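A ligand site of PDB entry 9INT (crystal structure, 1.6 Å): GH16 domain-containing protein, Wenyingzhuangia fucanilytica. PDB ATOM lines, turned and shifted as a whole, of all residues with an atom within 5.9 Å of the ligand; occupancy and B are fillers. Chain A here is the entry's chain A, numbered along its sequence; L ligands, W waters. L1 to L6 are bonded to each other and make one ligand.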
ATOM      1  N   GLN A  82      11.092 -18.204 -21.422  1.00  0.00           N
ATOM      2  CA  GLN A  82      10.789 -19.172 -22.463  1.00  0.00           C
ATOM      3  C   GLN A  82      11.297 -20.542 -22.035  1.00  0.00           C
ATOM      4  O   GLN A  82      12.418 -20.666 -21.527  1.00  0.00           O
ATOM      5  CB  GLN A  82      11.433 -18.747 -23.781  1.00  0.00           C
ATOM      6  CG  GLN A  82      10.981 -19.575 -24.964  1.00  0.00           C
ATOM      7  CD  GLN A  82       9.651 -19.112 -25.510  1.00  0.00           C
ATOM      8  OE1 GLN A  82       9.282 -17.947 -25.376  1.00  0.00           O
ATOM      9  NE2 GLN A  82       8.917 -20.017 -26.138  1.00  0.00           N
ATOM     10  N   SER A  83      10.455 -21.556 -22.170  1.00  0.00           N
ATOM     11  CA  SER A  83      10.780 -22.940 -21.805  1.00  0.00           C
ATOM     12  C   SER A  83      11.147 -23.095 -20.335  1.00  0.00           C
ATOM     13  O   SER A  83      11.726 -24.116 -19.963  1.00  0.00           O
ATOM     14  CB  SER A  83      11.923 -23.482 -22.668  1.00  0.00           C
ATOM     15  OG  SER A  83      11.469 -23.816 -23.962  1.00  0.00           O
ATOM     16  N   ARG A  84      10.830 -22.115 -19.488  1.00  0.00           N
ATOM     17  CA  ARG A  84      11.184 -22.150 -18.069  1.00  0.00           C
ATOM     18  C   ARG A  84      12.684 -22.373 -17.871  1.00  0.00           C
ATOM     19  O   ARG A  84      13.118 -22.957 -16.876  1.00  0.00           O
ATOM     20  CB  ARG A  84      10.366 -23.213 -17.325  1.00  0.00           C
ATOM     21  CG  ARG A  84       8.922 -22.791 -17.085  1.00  0.00           C
ATOM     22  CD  ARG A  84       8.017 -23.924 -16.576  1.00  0.00           C
ATOM     23  NE  ARG A  84       8.673 -24.842 -15.652  1.00  0.00           N
ATOM     24  CZ  ARG A  84       8.199 -25.170 -14.457  1.00  0.00           C
ATOM     25  NH1 ARG A  84       7.139 -24.561 -13.939  1.00  0.00           N
ATOM     26  NH2 ARG A  84       8.809 -26.129 -13.761  1.00  0.00           N
ATOM     27  N   PHE A  85      13.487 -21.859 -18.809  1.00  0.00           N
ATOM     28  CA  PHE A  85      14.926 -22.122 -18.865  1.00  0.00           C
ATOM     29  C   PHE A  85      15.667 -20.934 -18.260  1.00  0.00           C
ATOM     30  O   PHE A  85      15.823 -19.892 -18.910  1.00  0.00           O
ATOM     31  CB  PHE A  85      15.317 -22.381 -20.306  1.00  0.00           C
ATOM     32  CG  PHE A  85      16.770 -22.718 -20.535  1.00  0.00           C
ATOM     33  CD1 PHE A  85      17.515 -23.399 -19.581  1.00  0.00           C
ATOM     34  CD2 PHE A  85      17.362 -22.399 -21.750  1.00  0.00           C
ATOM     35  CE1 PHE A  85      18.854 -23.711 -19.821  1.00  0.00           C
ATOM     36  CE2 PHE A  85      18.689 -22.712 -22.002  1.00  0.00           C
ATOM     37  CZ  PHE A  85      19.435 -23.386 -21.041  1.00  0.00           C
ATOM     38  N   ARG A  88      21.922 -22.488 -17.997  1.00  0.00           N
ATOM     39  CA  ARG A  88      22.580 -23.772 -17.811  1.00  0.00           C
ATOM     40  C   ARG A  88      23.695 -23.583 -16.786  1.00  0.00           C
ATOM     41  O   ARG A  88      24.647 -22.840 -17.022  1.00  0.00           O
ATOM     42  CB  ARG A  88      23.139 -24.292 -19.145  1.00  0.00           C
ATOM     43  CG  ARG A  88      23.774 -25.677 -19.053  1.00  0.00           C
ATOM     44  CD  ARG A  88      24.014 -26.272 -20.426  1.00  0.00           C
ATOM     45  NE  ARG A  88      22.793 -26.340 -21.215  1.00  0.00           N
ATOM     46  CZ  ARG A  88      21.896 -27.317 -21.119  1.00  0.00           C
ATOM     47  NH1 ARG A  88      22.056 -28.316 -20.263  1.00  0.00           N
ATOM     48  NH2 ARG A  88      20.806 -27.281 -21.888  1.00  0.00           N
ATOM     49  N   THR A 167      29.289 -20.858 -24.714  1.00  0.00           N
ATOM     50  CA  THR A 167      28.674 -21.020 -26.022  1.00  0.00           C
ATOM     51  C   THR A 167      28.218 -19.679 -26.572  1.00  0.00           C
ATOM     52  O   THR A 167      28.004 -18.712 -25.842  1.00  0.00           O
ATOM     53  CB  THR A 167      27.459 -21.938 -26.005  1.00  0.00           C
ATOM     54  OG1 THR A 167      26.453 -21.364 -25.166  1.00  0.00           O
ATOM     55  CG2 THR A 167      27.847 -23.332 -25.507  1.00  0.00           C
ATOM     56  N   SER A 169      25.125 -19.348 -29.372  1.00  0.00           N
ATOM     57  CA  SER A 169      24.239 -20.267 -30.068  1.00  0.00           C
ATOM     58  C   SER A 169      23.098 -19.531 -30.765  1.00  0.00           C
ATOM     59  O   SER A 169      22.701 -18.434 -30.381  1.00  0.00           O
ATOM     60  CB  SER A 169      23.685 -21.324 -29.130  1.00  0.00           C
ATOM     61  OG  SER A 169      24.763 -22.029 -28.559  1.00  0.00           O
ATOM     62  N   TRP A 171      19.430 -20.813 -32.361  1.00  0.00           N
ATOM     63  CA  TRP A 171      18.656 -22.041 -32.308  1.00  0.00           C
ATOM     64  C   TRP A 171      17.168 -21.722 -32.231  1.00  0.00           C
ATOM     65  O   TRP A 171      16.758 -20.562 -32.290  1.00  0.00           O
ATOM     66  CB  TRP A 171      19.106 -22.934 -31.151  1.00  0.00           C
ATOM     67  CG  TRP A 171      19.248 -22.284 -29.784  1.00  0.00           C
ATOM     68  CD1 TRP A 171      20.150 -21.328 -29.422  1.00  0.00           C
ATOM     69  CD2 TRP A 171      18.508 -22.615 -28.610  1.00  0.00           C
ATOM     70  NE1 TRP A 171      20.006 -21.027 -28.072  1.00  0.00           N
ATOM     71  CE2 TRP A 171      19.008 -21.810 -27.570  1.00  0.00           C
ATOM     72  CE3 TRP A 171      17.476 -23.523 -28.336  1.00  0.00           C
ATOM     73  CZ2 TRP A 171      18.505 -21.897 -26.261  1.00  0.00           C
ATOM     74  CZ3 TRP A 171      16.967 -23.582 -27.055  1.00  0.00           C
ATOM     75  CH2 TRP A 171      17.485 -22.777 -26.032  1.00  0.00           C
ATOM     76  N   THR A 173      13.075 -23.272 -30.778  1.00  0.00           N
ATOM     77  CA  THR A 173      12.194 -24.247 -30.147  1.00  0.00           C
ATOM     78  C   THR A 173      10.799 -24.077 -30.712  1.00  0.00           C
ATOM     79  O   THR A 173      10.414 -23.008 -31.189  1.00  0.00           O
ATOM     80  CB  THR A 173      12.114 -24.090 -28.626  1.00  0.00           C
ATOM     81  OG1 THR A 173      11.749 -22.753 -28.309  1.00  0.00           O
ATOM     82  CG2 THR A 173      13.458 -24.423 -27.970  1.00  0.00           C
ATOM     83  N   GLY A 174      10.051 -25.169 -30.659  1.00  0.00           N
ATOM     84  CA  GLY A 174       8.607 -25.099 -30.734  1.00  0.00           C
ATOM     85  C   GLY A 174       8.033 -25.863 -29.549  1.00  0.00           C
ATOM     86  O   GLY A 174       8.669 -26.759 -28.995  1.00  0.00           O
ATOM     87  N   LYS A 175       6.817 -25.480 -29.166  1.00  0.00           N
ATOM     88  CA  LYS A 175       6.246 -25.974 -27.916  1.00  0.00           C
ATOM     89  C   LYS A 175       5.947 -27.465 -28.042  1.00  0.00           C
ATOM     90  O   LYS A 175       5.081 -27.868 -28.831  1.00  0.00           O
ATOM     91  CB  LYS A 175       4.982 -25.197 -27.562  1.00  0.00           C
ATOM     92  CG  LYS A 175       4.300 -25.737 -26.321  1.00  0.00           C
ATOM     93  CD  LYS A 175       3.091 -24.908 -25.928  1.00  0.00           C
ATOM     94  CE  LYS A 175       2.338 -25.580 -24.773  1.00  0.00           C
ATOM     95  NZ  LYS A 175       0.897 -25.197 -24.769  1.00  0.00           N
ATOM     96  N   ASN A 176       6.660 -28.270 -27.245  1.00  0.00           N
ATOM     97  CA  ASN A 176       6.629 -29.729 -27.279  1.00  0.00           C
ATOM     98  C   ASN A 176       6.576 -30.299 -28.699  1.00  0.00           C
ATOM     99  O   ASN A 176       5.905 -31.296 -28.962  1.00  0.00           O
ATOM    100  CB  ASN A 176       5.478 -30.263 -26.421  1.00  0.00           C
ATOM    101  CG  ASN A 176       5.416 -29.606 -25.064  1.00  0.00           C
ATOM    102  OD1 ASN A 176       4.369 -29.146 -24.624  1.00  0.00           O
ATOM    103  ND2 ASN A 176       6.570 -29.542 -24.379  1.00  0.00           N
ATOM    104  N   THR A 177       7.321 -29.681 -29.607  1.00  0.00           N
ATOM    105  CA  THR A 177       7.498 -30.248 -30.928  1.00  0.00           C
ATOM    106  C   THR A 177       8.962 -30.605 -31.094  1.00  0.00           C
ATOM    107  O   THR A 177       9.354 -31.756 -30.896  1.00  0.00           O
ATOM    108  CB  THR A 177       7.016 -29.278 -32.017  1.00  0.00           C
ATOM    109  OG1 THR A 177       7.625 -27.995 -31.829  1.00  0.00           O
ATOM    110  CG2 THR A 177       5.521 -29.136 -31.956  1.00  0.00           C
ATOM    111  N   SER A 178       9.795 -29.620 -31.394  1.00  0.00           N
ATOM    112  CA  SER A 178      11.186 -29.932 -31.686  1.00  0.00           C
ATOM    113  C   SER A 178      12.029 -28.676 -31.499  1.00  0.00           C
ATOM    114  O   SER A 178      11.536 -27.604 -31.149  1.00  0.00           O
ATOM    115  CB  SER A 178      11.348 -30.494 -33.097  1.00  0.00           C
ATOM    116  OG  SER A 178      10.908 -29.555 -34.057  1.00  0.00           O
ATOM    117  N   GLU A 179      13.319 -28.849 -31.763  1.00  0.00           N
ATOM    118  CA  GLU A 179      14.296 -27.795 -31.601  1.00  0.00           C
ATOM    119  C   GLU A 179      15.381 -28.023 -32.640  1.00  0.00           C
ATOM    120  O   GLU A 179      15.877 -29.134 -32.790  1.00  0.00           O
ATOM    121  CB  GLU A 179      14.883 -27.822 -30.191  1.00  0.00           C
ATOM    122  CG  GLU A 179      16.251 -27.272 -30.089  1.00  0.00           C
ATOM    123  CD  GLU A 179      16.815 -27.336 -28.697  1.00  0.00           C
ATOM    124  OE1 GLU A 179      16.162 -27.895 -27.775  1.00  0.00           O
ATOM    125  OE2 GLU A 179      17.914 -26.794 -28.508  1.00  0.00           O
ATOM    126  N   ASP A 181      19.083 -26.623 -33.417  1.00  0.00           N
ATOM    127  CA  ASP A 181      20.222 -25.786 -33.047  1.00  0.00           C
ATOM    128  C   ASP A 181      21.010 -25.533 -34.321  1.00  0.00           C
ATOM    129  O   ASP A 181      21.810 -26.376 -34.733  1.00  0.00           O
ATOM    130  CB  ASP A 181      21.087 -26.440 -31.977  1.00  0.00           C
ATOM    131  CG  ASP A 181      20.294 -26.808 -30.758  1.00  0.00           C
ATOM    132  OD1 ASP A 181      19.297 -26.107 -30.461  1.00  0.00           O
ATOM    133  OD2 ASP A 181      20.652 -27.818 -30.121  1.00  0.00           O
ATOM    134  N   GLU A 184      25.727 -24.200 -32.187  1.00  0.00           N
ATOM    135  CA  GLU A 184      26.333 -23.875 -30.903  1.00  0.00           C
ATOM    136  C   GLU A 184      27.811 -23.681 -31.184  1.00  0.00           C
ATOM    137  O   GLU A 184      28.491 -24.621 -31.610  1.00  0.00           O
ATOM    138  CB  GLU A 184      26.138 -24.983 -29.887  1.00  0.00           C
ATOM    139  CG  GLU A 184      24.705 -25.303 -29.596  1.00  0.00           C
ATOM    140  CD  GLU A 184      24.600 -26.537 -28.735  1.00  0.00           C
ATOM    141  OE1 GLU A 184      24.124 -26.414 -27.592  1.00  0.00           O
ATOM    142  OE2 GLU A 184      25.050 -27.626 -29.164  1.00  0.00           O
ATOM    143  N   ASN A 202      22.321 -29.335 -34.150  1.00  0.00           N
ATOM    144  CA  ASN A 202      21.514 -30.408 -33.586  1.00  0.00           C
ATOM    145  C   ASN A 202      20.070 -30.272 -34.021  1.00  0.00           C
ATOM    146  O   ASN A 202      19.572 -29.161 -34.251  1.00  0.00           O
ATOM    147  CB  ASN A 202      21.502 -30.411 -32.051  1.00  0.00           C
ATOM    148  CG  ASN A 202      22.871 -30.306 -31.466  1.00  0.00           C
ATOM    149  OD1 ASN A 202      23.731 -31.158 -31.702  1.00  0.00           O
ATOM    150  ND2 ASN A 202      23.088 -29.260 -30.686  1.00  0.00           N
ATOM    151  N   ILE A 204      16.522 -31.805 -32.205  1.00  0.00           N
ATOM    152  CA  ILE A 204      16.064 -32.402 -30.964  1.00  0.00           C
ATOM    153  C   ILE A 204      14.549 -32.524 -31.016  1.00  0.00           C
ATOM    154  O   ILE A 204      13.866 -31.607 -31.484  1.00  0.00           O
ATOM    155  CB  ILE A 204      16.519 -31.567 -29.759  1.00  0.00           C
ATOM    156  CG1 ILE A 204      18.040 -31.663 -29.654  1.00  0.00           C
ATOM    157  CG2 ILE A 204      15.833 -32.036 -28.462  1.00  0.00           C
ATOM    158  CD1 ILE A 204      18.629 -30.692 -28.653  1.00  0.00           C
ATOM    159  N   TRP A 206      11.101 -32.727 -28.952  1.00  0.00           N
ATOM    160  CA  TRP A 206      10.481 -32.444 -27.668  1.00  0.00           C
ATOM    161  C   TRP A 206       9.076 -33.041 -27.569  1.00  0.00           C
ATOM    162  O   TRP A 206       8.292 -32.636 -26.712  1.00  0.00           O
ATOM    163  CB  TRP A 206      10.451 -30.927 -27.438  1.00  0.00           C
ATOM    164  CG  TRP A 206      11.795 -30.374 -27.117  1.00  0.00           C
ATOM    165  CD1 TRP A 206      12.554 -29.526 -27.890  1.00  0.00           C
ATOM    166  CD2 TRP A 206      12.563 -30.633 -25.940  1.00  0.00           C
ATOM    167  NE1 TRP A 206      13.744 -29.249 -27.259  1.00  0.00           N
ATOM    168  CE2 TRP A 206      13.778 -29.922 -26.060  1.00  0.00           C
ATOM    169  CE3 TRP A 206      12.349 -31.406 -24.792  1.00  0.00           C
ATOM    170  CZ2 TRP A 206      14.762 -29.957 -25.073  1.00  0.00           C
ATOM    171  CZ3 TRP A 206      13.331 -31.435 -23.811  1.00  0.00           C
ATOM    172  CH2 TRP A 206      14.522 -30.711 -23.957  1.00  0.00           C
ATOM    173  N   PHE A 214      13.562 -36.431 -26.878  1.00  0.00           N
ATOM    174  CA  PHE A 214      14.791 -36.179 -26.138  1.00  0.00           C
ATOM    175  C   PHE A 214      14.819 -36.913 -24.801  1.00  0.00           C
ATOM    176  O   PHE A 214      15.867 -37.395 -24.373  1.00  0.00           O
ATOM    177  CB  PHE A 214      14.972 -34.677 -25.921  1.00  0.00           C
ATOM    178  CG  PHE A 214      16.274 -34.332 -25.273  1.00  0.00           C
ATOM    179  CD1 PHE A 214      17.454 -34.361 -25.995  1.00  0.00           C
ATOM    180  CD2 PHE A 214      16.307 -33.941 -23.940  1.00  0.00           C
ATOM    181  CE1 PHE A 214      18.656 -34.035 -25.403  1.00  0.00           C
ATOM    182  CE2 PHE A 214      17.511 -33.614 -23.334  1.00  0.00           C
ATOM    183  CZ  PHE A 214      18.689 -33.651 -24.076  1.00  0.00           C
ATOM    184  N   TRP A 284      10.152 -20.484 -32.499  1.00  0.00           N
ATOM    185  CA  TRP A 284      10.790 -19.266 -32.027  1.00  0.00           C
ATOM    186  C   TRP A 284      12.282 -19.354 -32.275  1.00  0.00           C
ATOM    187  O   TRP A 284      12.872 -20.444 -32.226  1.00  0.00           O
ATOM    188  CB  TRP A 284      10.583 -19.085 -30.528  1.00  0.00           C
ATOM    189  CG  TRP A 284       9.184 -18.948 -30.067  1.00  0.00           C
ATOM    190  CD1 TRP A 284       8.411 -17.821 -30.117  1.00  0.00           C
ATOM    191  CD2 TRP A 284       8.385 -19.955 -29.442  1.00  0.00           C
ATOM    192  NE1 TRP A 284       7.170 -18.073 -29.572  1.00  0.00           N
ATOM    193  CE2 TRP A 284       7.138 -19.384 -29.151  1.00  0.00           C
ATOM    194  CE3 TRP A 284       8.613 -21.308 -29.113  1.00  0.00           C
ATOM    195  CZ2 TRP A 284       6.102 -20.102 -28.551  1.00  0.00           C
ATOM    196  CZ3 TRP A 284       7.578 -22.019 -28.506  1.00  0.00           C
ATOM    197  CH2 TRP A 284       6.347 -21.419 -28.233  1.00  0.00           C
ATOM    198  N   TRP A 286      16.056 -18.314 -30.949  1.00  0.00           N
ATOM    199  CA  TRP A 286      16.853 -17.963 -29.790  1.00  0.00           C
ATOM    200  C   TRP A 286      18.253 -17.555 -30.199  1.00  0.00           C
ATOM    201  O   TRP A 286      18.859 -18.179 -31.079  1.00  0.00           O
ATOM    202  CB  TRP A 286      17.013 -19.152 -28.851  1.00  0.00           C
ATOM    203  CG  TRP A 286      15.824 -19.777 -28.242  1.00  0.00           C
ATOM    204  CD1 TRP A 286      14.788 -20.409 -28.870  1.00  0.00           C
ATOM    205  CD2 TRP A 286      15.625 -19.973 -26.830  1.00  0.00           C
ATOM    206  NE1 TRP A 286      13.934 -20.946 -27.931  1.00  0.00           N
ATOM    207  CE2 TRP A 286      14.426 -20.704 -26.676  1.00  0.00           C
ATOM    208  CE3 TRP A 286      16.335 -19.583 -25.700  1.00  0.00           C
ATOM    209  CZ2 TRP A 286      13.922 -21.047 -25.418  1.00  0.00           C
ATOM    210  CZ3 TRP A 286      15.840 -19.919 -24.451  1.00  0.00           C
ATOM    211  CH2 TRP A 286      14.636 -20.651 -24.325  1.00  0.00           C
ATOM    212  N   ASP A 288      21.653 -17.228 -27.635  1.00  0.00           N
ATOM    213  CA  ASP A 288      22.063 -17.185 -26.234  1.00  0.00           C
ATOM    214  C   ASP A 288      23.519 -17.586 -26.089  1.00  0.00           C
ATOM    215  O   ASP A 288      24.202 -17.926 -27.060  1.00  0.00           O
ATOM    216  CB  ASP A 288      21.128 -18.029 -25.354  1.00  0.00           C
ATOM    217  CG  ASP A 288      21.467 -19.510 -25.298  1.00  0.00           C
ATOM    218  OD1 ASP A 288      22.140 -20.075 -26.190  1.00  0.00           O
ATOM    219  OD2 ASP A 288      21.031 -20.124 -24.303  1.00  0.00           O
ATOM    220  N   GLU A 290      25.737 -19.851 -22.933  1.00  0.00           N
ATOM    221  CA  GLU A 290      25.564 -20.737 -21.803  1.00  0.00           C
ATOM    222  C   GLU A 290      26.923 -21.293 -21.410  1.00  0.00           C
ATOM    223  O   GLU A 290      27.781 -21.470 -22.270  1.00  0.00           O
ATOM    224  CB  GLU A 290      24.659 -21.927 -22.167  1.00  0.00           C
ATOM    225  CG  GLU A 290      23.235 -21.556 -22.502  1.00  0.00           C
ATOM    226  CD  GLU A 290      22.450 -22.731 -23.058  1.00  0.00           C
ATOM    227  OE1 GLU A 290      22.756 -23.875 -22.710  1.00  0.00           O
ATOM    228  OE2 GLU A 290      21.505 -22.499 -23.834  1.00  0.00           O
ATOM    229  N   PHE A 292      28.669 -24.627 -20.726  1.00  0.00           N
ATOM    230  CA  PHE A 292      28.594 -26.075 -20.839  1.00  0.00           C
ATOM    231  C   PHE A 292      29.666 -26.589 -19.899  1.00  0.00           C
ATOM    232  O   PHE A 292      30.841 -26.634 -20.283  1.00  0.00           O
ATOM    233  CB  PHE A 292      28.880 -26.534 -22.273  1.00  0.00           C
ATOM    234  CG  PHE A 292      27.720 -26.426 -23.212  1.00  0.00           C
ATOM    235  CD1 PHE A 292      27.754 -27.089 -24.428  1.00  0.00           C
ATOM    236  CD2 PHE A 292      26.618 -25.638 -22.921  1.00  0.00           C
ATOM    237  CE1 PHE A 292      26.695 -27.005 -25.311  1.00  0.00           C
ATOM    238  CE2 PHE A 292      25.559 -25.546 -23.796  1.00  0.00           C
ATOM    239  CZ  PHE A 292      25.598 -26.230 -24.992  1.00  0.00           C
HETATM  240  C1  LIG L   1      20.381 -27.514 -27.009  1.00  0.00           C
HETATM  241  C2  LIG L   1      19.598 -27.717 -25.702  1.00  0.00           C
HETATM  242  C3  LIG L   1      19.050 -26.404 -25.204  1.00  0.00           C
HETATM  243  C4  LIG L   1      20.034 -25.302 -25.181  1.00  0.00           C
HETATM  244  C5  LIG L   1      20.663 -25.177 -26.576  1.00  0.00           C
HETATM  245  C6  LIG L   1      21.632 -24.056 -26.701  1.00  0.00           C
HETATM  246  O1  LIG L   1      21.040 -28.645 -27.407  1.00  0.00           O
HETATM  247  O2  LIG L   1      18.541 -28.648 -25.954  1.00  0.00           O
HETATM  248  O3  LIG L   1      18.505 -26.613 -23.864  1.00  0.00           O
HETATM  249  O4  LIG L   1      21.037 -25.599 -24.184  1.00  0.00           O
HETATM  250  O5  LIG L   1      21.365 -26.453 -26.870  1.00  0.00           O
HETATM  251  O6  LIG L   1      22.840 -24.437 -26.080  1.00  0.00           O
HETATM  252  C1  LG2 L   2      16.944 -26.078 -22.153  1.00  0.00           C
HETATM  253  C2  LG2 L   2      14.792 -26.785 -22.862  1.00  0.00           C
HETATM  254  C3  LG2 L   2      14.924 -26.504 -24.107  1.00  0.00           C
HETATM  255  C4  LG2 L   2      14.716 -24.935 -24.215  1.00  0.00           C
HETATM  256  O1  LG2 L   2      13.261 -26.524 -22.381  1.00  0.00           O
HETATM  257  O2  LG2 L   2      16.306 -26.783 -24.577  1.00  0.00           O
HETATM  258  O3  LG2 L   2      15.179 -24.520 -22.731  1.00  0.00           O
HETATM  259  C5  LG2 L   2      15.510 -25.906 -22.088  1.00  0.00           C
HETATM  260  O4  LG2 L   2      17.257 -27.347 -21.660  1.00  0.00           O
HETATM  261  C6  LG2 L   2      17.424 -26.031 -23.737  1.00  0.00           C
HETATM  262  C1  LG3 L   3      12.332 -27.392 -22.892  1.00  0.00           C
HETATM  263  C2  LG3 L   3      11.173 -27.301 -21.903  1.00  0.00           C
HETATM  264  C3  LG3 L   3       9.870 -27.835 -22.410  1.00  0.00           C
HETATM  265  C4  LG3 L   3       9.570 -27.386 -23.789  1.00  0.00           C
HETATM  266  C5  LG3 L   3      10.753 -27.610 -24.715  1.00  0.00           C
HETATM  267  C6  LG3 L   3      10.543 -27.045 -26.084  1.00  0.00           C
HETATM  268  O1  LG3 L   3      11.542 -28.005 -20.715  1.00  0.00           O
HETATM  269  O2  LG3 L   3       8.888 -27.272 -21.488  1.00  0.00           O
HETATM  270  O3  LG3 L   3       9.419 -25.961 -23.696  1.00  0.00           O
HETATM  271  O4  LG3 L   3      11.893 -26.855 -24.172  1.00  0.00           O
HETATM  272  O5  LG3 L   3       9.475 -27.720 -26.662  1.00  0.00           O
HETATM  273  S1  LG3 L   3       7.976 -25.330 -24.156  1.00  0.00           S
HETATM  274  O6  LG3 L   3       7.733 -24.191 -23.195  1.00  0.00           O
HETATM  275  O7  LG3 L   3       6.898 -26.371 -24.129  1.00  0.00           O
HETATM  276  O8  LG3 L   3       8.122 -24.704 -25.504  1.00  0.00           O
HETATM  277  C1  LG4 L   4       6.830 -27.252 -20.308  1.00  0.00           C
HETATM  278  C2  LG4 L   4       6.765 -29.128 -18.952  1.00  0.00           C
HETATM  279  C3  LG4 L   4       7.332 -29.922 -19.794  1.00  0.00           C
HETATM  280  C4  LG4 L   4       6.186 -30.233 -20.847  1.00  0.00           C
HETATM  281  O1  LG4 L   4       5.752 -30.082 -18.078  1.00  0.00           O
HETATM  282  O2  LG4 L   4       8.442 -29.274 -20.505  1.00  0.00           O
HETATM  283  O3  LG4 L   4       5.196 -28.982 -20.649  1.00  0.00           O
HETATM  284  C5  LG4 L   4       6.038 -28.193 -19.564  1.00  0.00           C
HETATM  285  O4  LG4 L   4       7.548 -26.497 -19.374  1.00  0.00           O
HETATM  286  C6  LG4 L   4       7.919 -28.024 -21.299  1.00  0.00           C
HETATM  287  C1  LG5 L   5       6.295 -30.347 -16.849  1.00  0.00           C
HETATM  288  C2  LG5 L   5       5.197 -31.000 -16.004  1.00  0.00           C
HETATM  289  C3  LG5 L   5       5.740 -31.271 -14.654  1.00  0.00           C
HETATM  290  C4  LG5 L   5       6.934 -32.130 -14.707  1.00  0.00           C
HETATM  291  C5  LG5 L   5       8.002 -31.551 -15.632  1.00  0.00           C
HETATM  292  C6  LG5 L   5       9.129 -32.513 -15.802  1.00  0.00           C
HETATM  293  O1  LG5 L   5       4.072 -30.117 -15.955  1.00  0.00           O
HETATM  294  O2  LG5 L   5       4.714 -31.972 -13.869  1.00  0.00           O
HETATM  295  O3  LG5 L   5       6.523 -33.371 -15.287  1.00  0.00           O
HETATM  296  O4  LG5 L   5       7.419 -31.281 -16.976  1.00  0.00           O
HETATM  297  O5  LG5 L   5      10.083 -31.893 -16.608  1.00  0.00           O
HETATM  298  S1  LG5 L   5       6.762 -34.749 -14.393  1.00  0.00           S
HETATM  299  O6  LG5 L   5       8.186 -34.849 -13.891  1.00  0.00           O
HETATM  300  O7  LG5 L   5       6.384 -35.881 -15.309  1.00  0.00           O
HETATM  301  O8  LG5 L   5       5.944 -34.713 -13.128  1.00  0.00           O
HETATM  302  C1  LG6 L   6       3.929 -32.564 -11.715  1.00  0.00           C
HETATM  303  C2  LG6 L   6       3.367 -30.557 -10.678  1.00  0.00           C
HETATM  304  C3  LG6 L   6       4.380 -29.808 -11.103  1.00  0.00           C
HETATM  305  C4  LG6 L   6       5.622 -30.247 -10.221  1.00  0.00           C
HETATM  306  O1  LG6 L   6       2.838 -29.929  -9.273  1.00  0.00           O
HETATM  307  O2  LG6 L   6       4.722 -30.088 -12.471  1.00  0.00           O
HETATM  308  O3  LG6 L   6       5.154 -31.762  -9.775  1.00  0.00           O
HETATM  309  C5  LG6 L   6       3.723 -31.829 -10.479  1.00  0.00           C
HETATM  310  O4  LG6 L   6       2.703 -32.758 -12.371  1.00  0.00           O
HETATM  311  C6  LG6 L   6       4.928 -31.712 -12.699  1.00  0.00           C
HETATM  312  O   HOH W   1       7.908 -24.260 -20.463  1.00  0.00           O
HETATM  313  O   HOH W   2       7.765 -21.121 -22.916  1.00  0.00           O
HETATM  314  O   HOH W   3       9.988 -27.303 -18.306  1.00  0.00           O
HETATM  315  O   HOH W   4      12.916 -26.089 -18.888  1.00  0.00           O
HETATM  316  O   HOH W   5      17.908 -29.495 -23.231  1.00  0.00           O
HETATM  317  O   HOH W   6      10.102 -22.815 -26.119  1.00  0.00           O
HETATM  318  O   HOH W   7      17.634 -27.070 -18.925  1.00  0.00           O
HETATM  319  O   HOH W   8      24.005 -21.954 -25.929  1.00  0.00           O
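CD of Arg 84 touches O4 of LG4 L4, at 3.8 Å.
CD2 of Phe 85 touches O3 of LG2 L2 (3.2 Å).
OG of Ser 169 touches O6 of LIG L1, at 3.95 Å.
CE2 of Trp 171 touches C6 of LIG L1 (3.6 Å).
CG2 of Thr 173 touches C4 of LG2 L2 (3.99 Å).
CA of Lys 175 touches O8 of LG3 L3, at 3.3 Å.
Asn 202 touches the ligand.
Ile 204 touches the ligand.
CB of Trp 206 touches O5 of LG3 L3, 3.4 Å away.
Phe 292 touches the ligand.
Hydrophobic or aromatic side chains that line the ligand: Phe 85, Trp 171, Ile 204, Trp 206 and Phe 292.
Within 4 Å of the ligand: Ser 83, Arg 84, Phe 85, Arg 88, Ser 169, Trp 171, Thr 173, Gly 174, Lys 175, Asn 176, Glu 179, Asp 181, Glu 184, Asn 202, Ile 204, Trp 206, Glu 290 and Phe 292.
Along chain A the residues within 4 Å of the ligand span positions 83 to 292.
The nearest printed residue that does not touch the ligand is Asp 288 (4.05 Å).
O of Asp 288 lies within hydrogen-bond range of N of Ser 169, at 2.9 Å.
The backbone NH of Trp 206 sits at hydrogen-bond distance from the backbone carbonyl oxygen of Thr 177, at 2.8 Å.
The side-chain carboxylate of Glu 290 lies close to the side-chain carboxylate of Asp 288, at 2.5 Å.
NE1 of Trp 286 is in hydrogen-bond range of OG1 of Thr 173.
The backbone carbonyl oxygen (O) of Asn 202 is in hydrogen-bond range of the backbone NH (N) of Asp 181 (2.7 Å).
The backbone carbonyl oxygen (O) of Glu 179 lies within hydrogen-bond range of the backbone NH (N) of Ile 204.
The side-chain carboxylate of Glu 290 is in salt-bridge range of the guanidinium group of Arg 88, 2.9 Å away.
N of Glu 290 is in hydrogen-bond range of OG1 of Thr 167 (2.8 Å).
Water W8 lies within hydrogen-bond range of OG1 of Thr 167, OD1 of Asp 288, OG of Ser 169, O6 of LIG L1 and OE2 of Glu 290.
Water W6 lies within hydrogen-bond range of the side-chain hydroxyl of Thr 173 (2.7 Å), the side-chain hydroxyl of Ser 83 (2.7 Å), an oxygen (O8) of LG3 L3 (2.8 Å) and the side-chain amide nitrogen of Gln 82 (3.0 Å).
Water W4 bridges the backbone carbonyl oxygen (O) of Ser 83 (2.5 Å) and an oxygen (O1) of LG3 L3 (3.0 Å).
Water W2 bridges N of Ser 83 (2.8 Å) and O6 of LG3 L3 (3.1 Å).
The side-chain carboxylate (OE1) of Glu 179 sits at hydrogen-bond distance from an oxygen (O2) of LIG L1, 3.1 Å away.
OE1 of Glu 290 lies within hydrogen-bond range of O4 of LIG L1, 2.8 Å away.
The side-chain hydroxyl of Ser 83 lies within hydrogen-bond range of an oxygen (O3) of LG3 L3 (3.0 Å).
The side-chain amide nitrogen (ND2) of Asn 176 lies within hydrogen-bond range of an oxygen (O7) of LG3 L3 (3.2 Å).
O5 of LG3 L3 sits at hydrogen-bond distance from O of Gly 174, 2.6 Å away.
The guanidinium group (NH2) of Arg 88 is in hydrogen-bond range of an oxygen (O4) of LIG L1.
OE1 of Glu 184 lies within hydrogen-bond range of O6 of LIG L1.
N of Asn 176 lies within hydrogen-bond range of O5 of LG3 L3 (2.9 Å).
An oxygen (O1) of LIG L1 is in hydrogen-bond range of the side-chain carboxylate (OD2) of Asp 181, 2.9 Å away.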
